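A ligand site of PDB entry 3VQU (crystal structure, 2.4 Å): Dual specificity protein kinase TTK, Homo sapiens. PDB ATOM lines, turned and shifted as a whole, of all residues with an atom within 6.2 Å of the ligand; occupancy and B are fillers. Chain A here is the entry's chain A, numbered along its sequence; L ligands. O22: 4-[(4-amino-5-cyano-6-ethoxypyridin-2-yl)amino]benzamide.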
ATOM      1  N   LYS A  14      12.634 -23.967 -20.914  1.00  0.00           N
ATOM      2  CA  LYS A  14      11.410 -24.364 -21.602  1.00  0.00           C
ATOM      3  C   LYS A  14      11.004 -23.298 -22.639  1.00  0.00           C
ATOM      4  O   LYS A  14      11.443 -22.151 -22.567  1.00  0.00           O
ATOM      5  CB  LYS A  14      10.320 -24.751 -20.602  1.00  0.00           C
ATOM      6  CG  LYS A  14       9.655 -23.575 -19.918  1.00  0.00           C
ATOM      7  CD  LYS A  14       8.230 -23.912 -19.493  1.00  0.00           C
ATOM      8  CE  LYS A  14       7.786 -23.048 -18.321  1.00  0.00           C
ATOM      9  N   ILE A  16       8.164 -20.839 -24.085  1.00  0.00           N
ATOM     10  CA  ILE A  16       7.058 -20.089 -23.495  1.00  0.00           C
ATOM     11  C   ILE A  16       6.252 -19.285 -24.511  1.00  0.00           C
ATOM     12  O   ILE A  16       5.289 -18.593 -24.148  1.00  0.00           O
ATOM     13  CB  ILE A  16       7.550 -19.164 -22.331  1.00  0.00           C
ATOM     14  CG1 ILE A  16       8.744 -18.308 -22.791  1.00  0.00           C
ATOM     15  CG2 ILE A  16       7.900 -19.996 -21.098  1.00  0.00           C
ATOM     16  CD1 ILE A  16       9.220 -17.284 -21.782  1.00  0.00           C
ATOM     17  N   GLY A  17       6.648 -19.370 -25.780  1.00  0.00           N
ATOM     18  CA  GLY A  17       5.968 -18.651 -26.863  1.00  0.00           C
ATOM     19  C   GLY A  17       6.341 -19.147 -28.252  1.00  0.00           C
ATOM     20  O   GLY A  17       7.408 -19.734 -28.439  1.00  0.00           O
ATOM     21  N   SER A  18       5.455 -18.909 -29.212  1.00  0.00           N
ATOM     22  CA  SER A  18       5.668 -19.304 -30.603  1.00  0.00           C
ATOM     23  C   SER A  18       4.951 -18.354 -31.569  1.00  0.00           C
ATOM     24  O   SER A  18       4.108 -17.563 -31.162  1.00  0.00           O
ATOM     25  CB  SER A  18       5.212 -20.747 -30.836  1.00  0.00           C
ATOM     26  OG  SER A  18       3.811 -20.820 -30.983  1.00  0.00           O
ATOM     27  N   VAL A  24       9.822 -18.110 -28.248  1.00  0.00           N
ATOM     28  CA  VAL A  24      10.316 -17.522 -26.999  1.00  0.00           C
ATOM     29  C   VAL A  24      10.654 -18.636 -25.997  1.00  0.00           C
ATOM     30  O   VAL A  24       9.842 -19.537 -25.767  1.00  0.00           O
ATOM     31  CB  VAL A  24       9.311 -16.511 -26.383  1.00  0.00           C
ATOM     32  CG1 VAL A  24       9.948 -15.737 -25.226  1.00  0.00           C
ATOM     33  CG2 VAL A  24       8.824 -15.523 -27.435  1.00  0.00           C
ATOM     34  N   GLN A  26      12.307 -19.781 -22.077  1.00  0.00           N
ATOM     35  CA  GLN A  26      12.698 -19.475 -20.711  1.00  0.00           C
ATOM     36  C   GLN A  26      14.095 -20.068 -20.483  1.00  0.00           C
ATOM     37  O   GLN A  26      14.272 -21.280 -20.518  1.00  0.00           O
ATOM     38  CB  GLN A  26      11.696 -20.061 -19.719  1.00  0.00           C
ATOM     39  CG  GLN A  26      11.817 -19.506 -18.299  1.00  0.00           C
ATOM     40  CD  GLN A  26      10.813 -20.130 -17.341  1.00  0.00           C
ATOM     41  OE1 GLN A  26      10.491 -21.317 -17.431  1.00  0.00           O
ATOM     42  NE2 GLN A  26      10.320 -19.333 -16.392  1.00  0.00           N
ATOM     43  N   ALA A  36      14.505 -14.158 -20.838  1.00  0.00           N
ATOM     44  CA  ALA A  36      13.651 -14.588 -21.941  1.00  0.00           C
ATOM     45  C   ALA A  36      14.328 -14.348 -23.280  1.00  0.00           C
ATOM     46  O   ALA A  36      14.665 -13.208 -23.619  1.00  0.00           O
ATOM     47  CB  ALA A  36      12.296 -13.884 -21.868  1.00  0.00           C
ATOM     48  N   ILE A  37      14.540 -15.421 -24.040  1.00  0.00           N
ATOM     49  CA  ILE A  37      15.186 -15.326 -25.351  1.00  0.00           C
ATOM     50  C   ILE A  37      14.191 -15.573 -26.476  1.00  0.00           C
ATOM     51  O   ILE A  37      13.537 -16.616 -26.538  1.00  0.00           O
ATOM     52  CB  ILE A  37      16.402 -16.278 -25.469  1.00  0.00           C
ATOM     53  CG1 ILE A  37      17.525 -15.834 -24.518  1.00  0.00           C
ATOM     54  CG2 ILE A  37      16.932 -16.318 -26.908  1.00  0.00           C
ATOM     55  CD1 ILE A  37      18.865 -16.514 -24.759  1.00  0.00           C
ATOM     56  N   LYS A  38      14.078 -14.589 -27.373  1.00  0.00           N
ATOM     57  CA  LYS A  38      13.201 -14.667 -28.532  1.00  0.00           C
ATOM     58  C   LYS A  38      13.999 -15.035 -29.786  1.00  0.00           C
ATOM     59  O   LYS A  38      14.884 -14.296 -30.212  1.00  0.00           O
ATOM     60  CB  LYS A  38      12.452 -13.332 -28.716  1.00  0.00           C
ATOM     61  CG  LYS A  38      11.408 -13.332 -29.818  1.00  0.00           C
ATOM     62  CD  LYS A  38      10.714 -11.984 -29.905  1.00  0.00           C
ATOM     63  CE  LYS A  38       9.636 -11.970 -30.973  1.00  0.00           C
ATOM     64  NZ  LYS A  38       8.796 -10.742 -30.899  1.00  0.00           N
ATOM     65  N   ILE A  71       9.359  -3.482 -21.368  1.00  0.00           N
ATOM     66  CA  ILE A  71      10.189  -4.676 -21.136  1.00  0.00           C
ATOM     67  C   ILE A  71      11.678  -4.413 -21.412  1.00  0.00           C
ATOM     68  O   ILE A  71      12.018  -3.655 -22.328  1.00  0.00           O
ATOM     69  CB  ILE A  71       9.659  -5.916 -21.909  1.00  0.00           C
ATOM     70  CG1 ILE A  71       9.752  -7.195 -21.068  1.00  0.00           C
ATOM     71  CG2 ILE A  71      10.364  -6.075 -23.257  1.00  0.00           C
ATOM     72  CD1 ILE A  71       8.783  -7.236 -19.903  1.00  0.00           C
ATOM     73  N   ARG A  72      12.536  -5.046 -20.621  1.00  0.00           N
ATOM     74  CA  ARG A  72      13.970  -4.816 -20.693  1.00  0.00           C
ATOM     75  C   ARG A  72      14.626  -5.682 -21.771  1.00  0.00           C
ATOM     76  O   ARG A  72      14.400  -6.886 -21.824  1.00  0.00           O
ATOM     77  CB  ARG A  72      14.623  -5.098 -19.328  1.00  0.00           C
ATOM     78  CG  ARG A  72      15.572  -4.005 -18.850  1.00  0.00           C
ATOM     79  CD  ARG A  72      14.888  -3.020 -17.893  1.00  0.00           C
ATOM     80  NE  ARG A  72      13.827  -2.243 -18.542  1.00  0.00           N
ATOM     81  CZ  ARG A  72      14.003  -1.054 -19.123  1.00  0.00           C
ATOM     82  NH1 ARG A  72      12.964  -0.431 -19.676  1.00  0.00           N
ATOM     83  NH2 ARG A  72      15.202  -0.490 -19.148  1.00  0.00           N
ATOM     84  N   MET A  87      16.039 -10.730 -23.125  1.00  0.00           N
ATOM     85  CA  MET A  87      15.183  -9.745 -22.471  1.00  0.00           C
ATOM     86  C   MET A  87      14.648 -10.243 -21.124  1.00  0.00           C
ATOM     87  O   MET A  87      14.802 -11.424 -20.782  1.00  0.00           O
ATOM     88  CB  MET A  87      14.009  -9.363 -23.388  1.00  0.00           C
ATOM     89  CG  MET A  87      13.851 -10.253 -24.617  1.00  0.00           C
ATOM     90  SD  MET A  87      12.377  -9.893 -25.584  1.00  0.00           S
ATOM     91  CE  MET A  87      12.455  -8.102 -25.701  1.00  0.00           C
ATOM     92  N   GLU A  88      14.046  -9.337 -20.361  1.00  0.00           N
ATOM     93  CA  GLU A  88      13.430  -9.664 -19.079  1.00  0.00           C
ATOM     94  C   GLU A  88      12.410 -10.796 -19.268  1.00  0.00           C
ATOM     95  O   GLU A  88      11.690 -10.828 -20.263  1.00  0.00           O
ATOM     96  CB  GLU A  88      12.758  -8.419 -18.488  1.00  0.00           C
ATOM     97  CG  GLU A  88      12.715  -8.384 -16.962  1.00  0.00           C
ATOM     98  CD  GLU A  88      12.040  -7.125 -16.421  1.00  0.00           C
ATOM     99  OE1 GLU A  88      11.792  -6.190 -17.201  1.00  0.00           O
ATOM    100  OE2 GLU A  88      11.754  -7.086 -15.210  1.00  0.00           O
ATOM    101  N   CYS A  89      12.377 -11.708 -18.297  1.00  0.00           N
ATOM    102  CA  CYS A  89      11.528 -12.905 -18.374  1.00  0.00           C
ATOM    103  C   CYS A  89      10.214 -12.754 -17.625  1.00  0.00           C
ATOM    104  O   CYS A  89       9.218 -13.382 -17.982  1.00  0.00           O
ATOM    105  CB  CYS A  89      12.290 -14.134 -17.866  1.00  0.00           C
ATOM    106  SG  CYS A  89      11.424 -15.702 -18.117  1.00  0.00           S
ATOM    107  N   GLY A  90      10.214 -11.916 -16.583  1.00  0.00           N
ATOM    108  CA  GLY A  90       9.025 -11.681 -15.780  1.00  0.00           C
ATOM    109  C   GLY A  90       8.472 -12.934 -15.133  1.00  0.00           C
ATOM    110  O   GLY A  90       9.160 -13.959 -15.062  1.00  0.00           O
ATOM    111  N   ASN A  91       7.232 -12.854 -14.667  1.00  0.00           N
ATOM    112  CA  ASN A  91       6.565 -13.973 -13.999  1.00  0.00           C
ATOM    113  C   ASN A  91       5.631 -14.728 -14.947  1.00  0.00           C
ATOM    114  O   ASN A  91       5.746 -15.947 -15.102  1.00  0.00           O
ATOM    115  CB  ASN A  91       5.811 -13.486 -12.762  1.00  0.00           C
ATOM    116  CG  ASN A  91       5.521 -14.601 -11.757  1.00  0.00           C
ATOM    117  OD1 ASN A  91       4.871 -15.594 -12.080  1.00  0.00           O
ATOM    118  ND2 ASN A  91       6.005 -14.417 -10.541  1.00  0.00           N
ATOM    119  N   ILE A  92       4.725 -13.986 -15.590  1.00  0.00           N
ATOM    120  CA  ILE A  92       3.745 -14.535 -16.520  1.00  0.00           C
ATOM    121  C   ILE A  92       3.027 -13.411 -17.273  1.00  0.00           C
ATOM    122  O   ILE A  92       2.937 -12.289 -16.759  1.00  0.00           O
ATOM    123  CB  ILE A  92       2.723 -15.487 -15.799  1.00  0.00           C
ATOM    124  CG1 ILE A  92       1.868 -16.258 -16.804  1.00  0.00           C
ATOM    125  CG2 ILE A  92       1.866 -14.703 -14.776  1.00  0.00           C
ATOM    126  CD1 ILE A  92       0.525 -16.738 -16.261  1.00  0.00           C
ATOM    127  N   ASP A  93       2.549 -13.697 -18.471  1.00  0.00           N
ATOM    128  CA  ASP A  93       1.799 -12.717 -19.263  1.00  0.00           C
ATOM    129  C   ASP A  93       0.399 -12.503 -18.686  1.00  0.00           C
ATOM    130  O   ASP A  93      -0.199 -13.432 -18.122  1.00  0.00           O
ATOM    131  CB  ASP A  93       1.729 -13.117 -20.742  1.00  0.00           C
ATOM    132  CG  ASP A  93       0.706 -14.212 -21.018  1.00  0.00           C
ATOM    133  OD1 ASP A  93      -0.331 -13.911 -21.638  1.00  0.00           O
ATOM    134  OD2 ASP A  93       0.939 -15.370 -20.594  1.00  0.00           O
ATOM    135  N   SER A  96      -2.635 -15.094 -19.590  1.00  0.00           N
ATOM    136  CA  SER A  96      -2.605 -16.391 -18.917  1.00  0.00           C
ATOM    137  C   SER A  96      -2.989 -16.266 -17.448  1.00  0.00           C
ATOM    138  O   SER A  96      -3.733 -17.099 -16.915  1.00  0.00           O
ATOM    139  CB  SER A  96      -1.231 -17.047 -19.055  1.00  0.00           C
ATOM    140  OG  SER A  96      -0.888 -17.232 -20.414  1.00  0.00           O
ATOM    141  N   ALA A 136      -2.220 -10.282 -23.639  1.00  0.00           N
ATOM    142  CA  ALA A 136      -1.027 -11.062 -23.981  1.00  0.00           C
ATOM    143  C   ALA A 136       0.188 -10.168 -24.261  1.00  0.00           C
ATOM    144  O   ALA A 136       1.325 -10.648 -24.284  1.00  0.00           O
ATOM    145  CB  ALA A 136      -1.313 -11.966 -25.173  1.00  0.00           C
ATOM    146  N   LEU A 139       3.293  -8.192 -19.494  1.00  0.00           N
ATOM    147  CA  LEU A 139       3.950  -9.195 -18.674  1.00  0.00           C
ATOM    148  C   LEU A 139       3.972  -8.791 -17.204  1.00  0.00           C
ATOM    149  O   LEU A 139       4.275  -7.637 -16.873  1.00  0.00           O
ATOM    150  CB  LEU A 139       5.379  -9.444 -19.173  1.00  0.00           C
ATOM    151  CG  LEU A 139       6.239 -10.508 -18.473  1.00  0.00           C
ATOM    152  CD1 LEU A 139       5.854 -11.908 -18.904  1.00  0.00           C
ATOM    153  CD2 LEU A 139       7.712 -10.254 -18.755  1.00  0.00           C
ATOM    154  N   ILE A 148       5.356  -5.749 -23.546  1.00  0.00           N
ATOM    155  CA  ILE A 148       6.279  -6.691 -24.189  1.00  0.00           C
ATOM    156  C   ILE A 148       6.717  -6.208 -25.581  1.00  0.00           C
ATOM    157  O   ILE A 148       7.909  -6.115 -25.867  1.00  0.00           O
ATOM    158  CB  ILE A 148       5.674  -8.116 -24.281  1.00  0.00           C
ATOM    159  CG1 ILE A 148       5.466  -8.705 -22.873  1.00  0.00           C
ATOM    160  CG2 ILE A 148       6.567  -9.032 -25.117  1.00  0.00           C
ATOM    161  CD1 ILE A 148       4.401  -9.787 -22.788  1.00  0.00           C
ATOM    162  N   MET A 156       3.115 -12.608 -31.560  1.00  0.00           N
ATOM    163  CA  MET A 156       3.302 -13.968 -31.075  1.00  0.00           C
ATOM    164  C   MET A 156       2.260 -14.308 -30.015  1.00  0.00           C
ATOM    165  O   MET A 156       1.423 -13.470 -29.668  1.00  0.00           O
ATOM    166  CB  MET A 156       4.658 -14.109 -30.385  1.00  0.00           C
ATOM    167  CG  MET A 156       5.861 -13.867 -31.283  1.00  0.00           C
ATOM    168  SD  MET A 156       7.272 -14.914 -30.873  1.00  0.00           S
ATOM    169  CE  MET A 156       6.512 -16.057 -29.714  1.00  0.00           C
ATOM    170  N   GLN A 157       2.305 -15.542 -29.523  1.00  0.00           N
ATOM    171  CA  GLN A 157       1.377 -15.999 -28.480  1.00  0.00           C
ATOM    172  C   GLN A 157       2.011 -16.891 -27.417  1.00  0.00           C
ATOM    173  O   GLN A 157       2.820 -17.776 -27.745  1.00  0.00           O
ATOM    174  CB  GLN A 157       0.222 -16.715 -29.192  1.00  0.00           C
ATOM    175  N   PRO A 158       1.660 -16.666 -26.138  1.00  0.00           N
ATOM    176  CA  PRO A 158       2.200 -17.441 -25.015  1.00  0.00           C
ATOM    177  C   PRO A 158       1.753 -18.893 -25.025  1.00  0.00           C
ATOM    178  O   PRO A 158       0.650 -19.199 -25.492  1.00  0.00           O
ATOM    179  CB  PRO A 158       1.638 -16.723 -23.781  1.00  0.00           C
ATOM    180  CG  PRO A 158       1.243 -15.365 -24.263  1.00  0.00           C
ATOM    181  CD  PRO A 158       0.778 -15.585 -25.672  1.00  0.00           C
ATOM    182  N   ASP A 159       2.607 -19.781 -24.500  1.00  0.00           N
ATOM    183  CA  ASP A 159       2.300 -21.213 -24.424  1.00  0.00           C
ATOM    184  C   ASP A 159       1.714 -21.576 -23.064  1.00  0.00           C
ATOM    185  O   ASP A 159       0.819 -22.417 -22.975  1.00  0.00           O
ATOM    186  CB  ASP A 159       3.565 -22.033 -24.697  1.00  0.00           C
ATOM    187  CG  ASP A 159       3.992 -22.010 -26.161  1.00  0.00           C
ATOM    188  OD1 ASP A 159       3.341 -21.305 -26.966  1.00  0.00           O
ATOM    189  OD2 ASP A 159       4.984 -22.685 -26.499  1.00  0.00           O
HETATM  190  O2  O22 L   1       4.453 -18.995 -18.707  1.00  0.00           O
HETATM  191  C15 O22 L   1       4.029 -17.933 -19.053  1.00  0.00           C
HETATM  192  N4  O22 L   1       2.749 -17.749 -19.119  1.00  0.00           N
HETATM  193  C12 O22 L   1       4.974 -16.857 -19.403  1.00  0.00           C
HETATM  194  C11 O22 L   1       4.853 -16.202 -20.596  1.00  0.00           C
HETATM  195  C10 O22 L   1       5.738 -15.204 -20.920  1.00  0.00           C
HETATM  196  C13 O22 L   1       5.976 -16.522 -18.544  1.00  0.00           C
HETATM  197  C14 O22 L   1       6.853 -15.529 -18.870  1.00  0.00           C
HETATM  198  C9  O22 L   1       6.748 -14.881 -20.062  1.00  0.00           C
HETATM  199  N3  O22 L   1       7.619 -13.924 -20.347  1.00  0.00           N
HETATM  200  C8  O22 L   1       7.880 -13.424 -21.554  1.00  0.00           C
HETATM  201  C7  O22 L   1       8.923 -12.545 -21.640  1.00  0.00           C
HETATM  202  C6  O22 L   1       9.287 -11.973 -22.813  1.00  0.00           C
HETATM  203  N2  O22 L   1      10.300 -11.122 -22.839  1.00  0.00           N
HETATM  204  C4  O22 L   1       8.546 -12.315 -24.004  1.00  0.00           C
HETATM  205  C5  O22 L   1       8.870 -11.802 -25.135  1.00  0.00           C
HETATM  206  N1  O22 L   1       9.159 -11.331 -26.134  1.00  0.00           N
HETATM  207  N5  O22 L   1       7.170 -13.757 -22.609  1.00  0.00           N
HETATM  208  C3  O22 L   1       7.434 -13.265 -23.809  1.00  0.00           C
HETATM  209  O1  O22 L   1       6.651 -13.684 -24.791  1.00  0.00           O
HETATM  210  C2  O22 L   1       5.591 -14.485 -24.387  1.00  0.00           C
HETATM  211  C1  O22 L   1       4.928 -14.954 -25.643  1.00  0.00           C
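The backbone carbonyl oxygen (O) of Arg 72 sits at hydrogen-bond distance from the backbone NH (N) of Glu 88 (2.9 Å).
OG of Ser 96 sits at hydrogen-bond distance from OD2 of Asp 93 (2.6 Å).
The backbone carbonyl oxygen (O) of Met 87 lies within hydrogen-bond range of the backbone NH (N) of Ala 36 (2.8 Å).
The backbone carbonyl oxygen of Val 24 sits at hydrogen-bond distance from the backbone NH of Ile 16, 2.7 Å away.
The backbone NH (N) of Val 24 lies within hydrogen-bond range of the backbone carbonyl oxygen (O) of Gly 17, 2.9 Å away.
N of Asp 159 sits at hydrogen-bond distance from O of Ile 16 (3.0 Å).
N of Gln 157 is in hydrogen-bond range of O of Ser 18.
N3 of the ligand sits at hydrogen-bond distance from O of Cys 89 (2.9 Å).
The backbone carbonyl oxygen (O) of Glu 88 is in hydrogen-bond range of a nitrogen (N2) of the ligand (2.9 Å).
N4 of the ligand sits at hydrogen-bond distance from OD2 of Asp 93, 3.3 Å away.
N2 of the ligand lies within hydrogen-bond range of SD of Met 87 (3.7 Å).
Ile 16 touches the ligand (CD1 to C9, 3.9 Å).
Val 24 touches the ligand (CG1 to C3, 3.8 Å).
Ala 36 touches the ligand (CB to N2, 3.5 Å).
Asn 91 touches the ligand.
CG1 of Ile 92 touches N4 of the ligand, 2.9 Å away.
OG of Ser 96 touches N4 of the ligand (3.9 Å).
Leu 139 touches the ligand.
Ile 148 touches the ligand (CG2 to C5, 3.6 Å).
Gln 157 touches the ligand (C to C1, 3.9 Å).
Pro 158 touches the ligand.
Hydrophobic or aromatic side chains within 4 Å of the ligand: Ile 16, Val 24, Ala 36, Met 87, Ile 92, Leu 139, Ile 148 and Pro 158.
Within 4 Å of the ligand: Ile 16, Val 24, Ala 36, Met 87, Glu 88, Cys 89, Asn 91, Ile 92, Asp 93, Ser 96, Leu 139, Ile 148, Gln 157 and Pro 158.
The nearest printed residue that does not touch the ligand is Gly 17 (4.03 Å).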
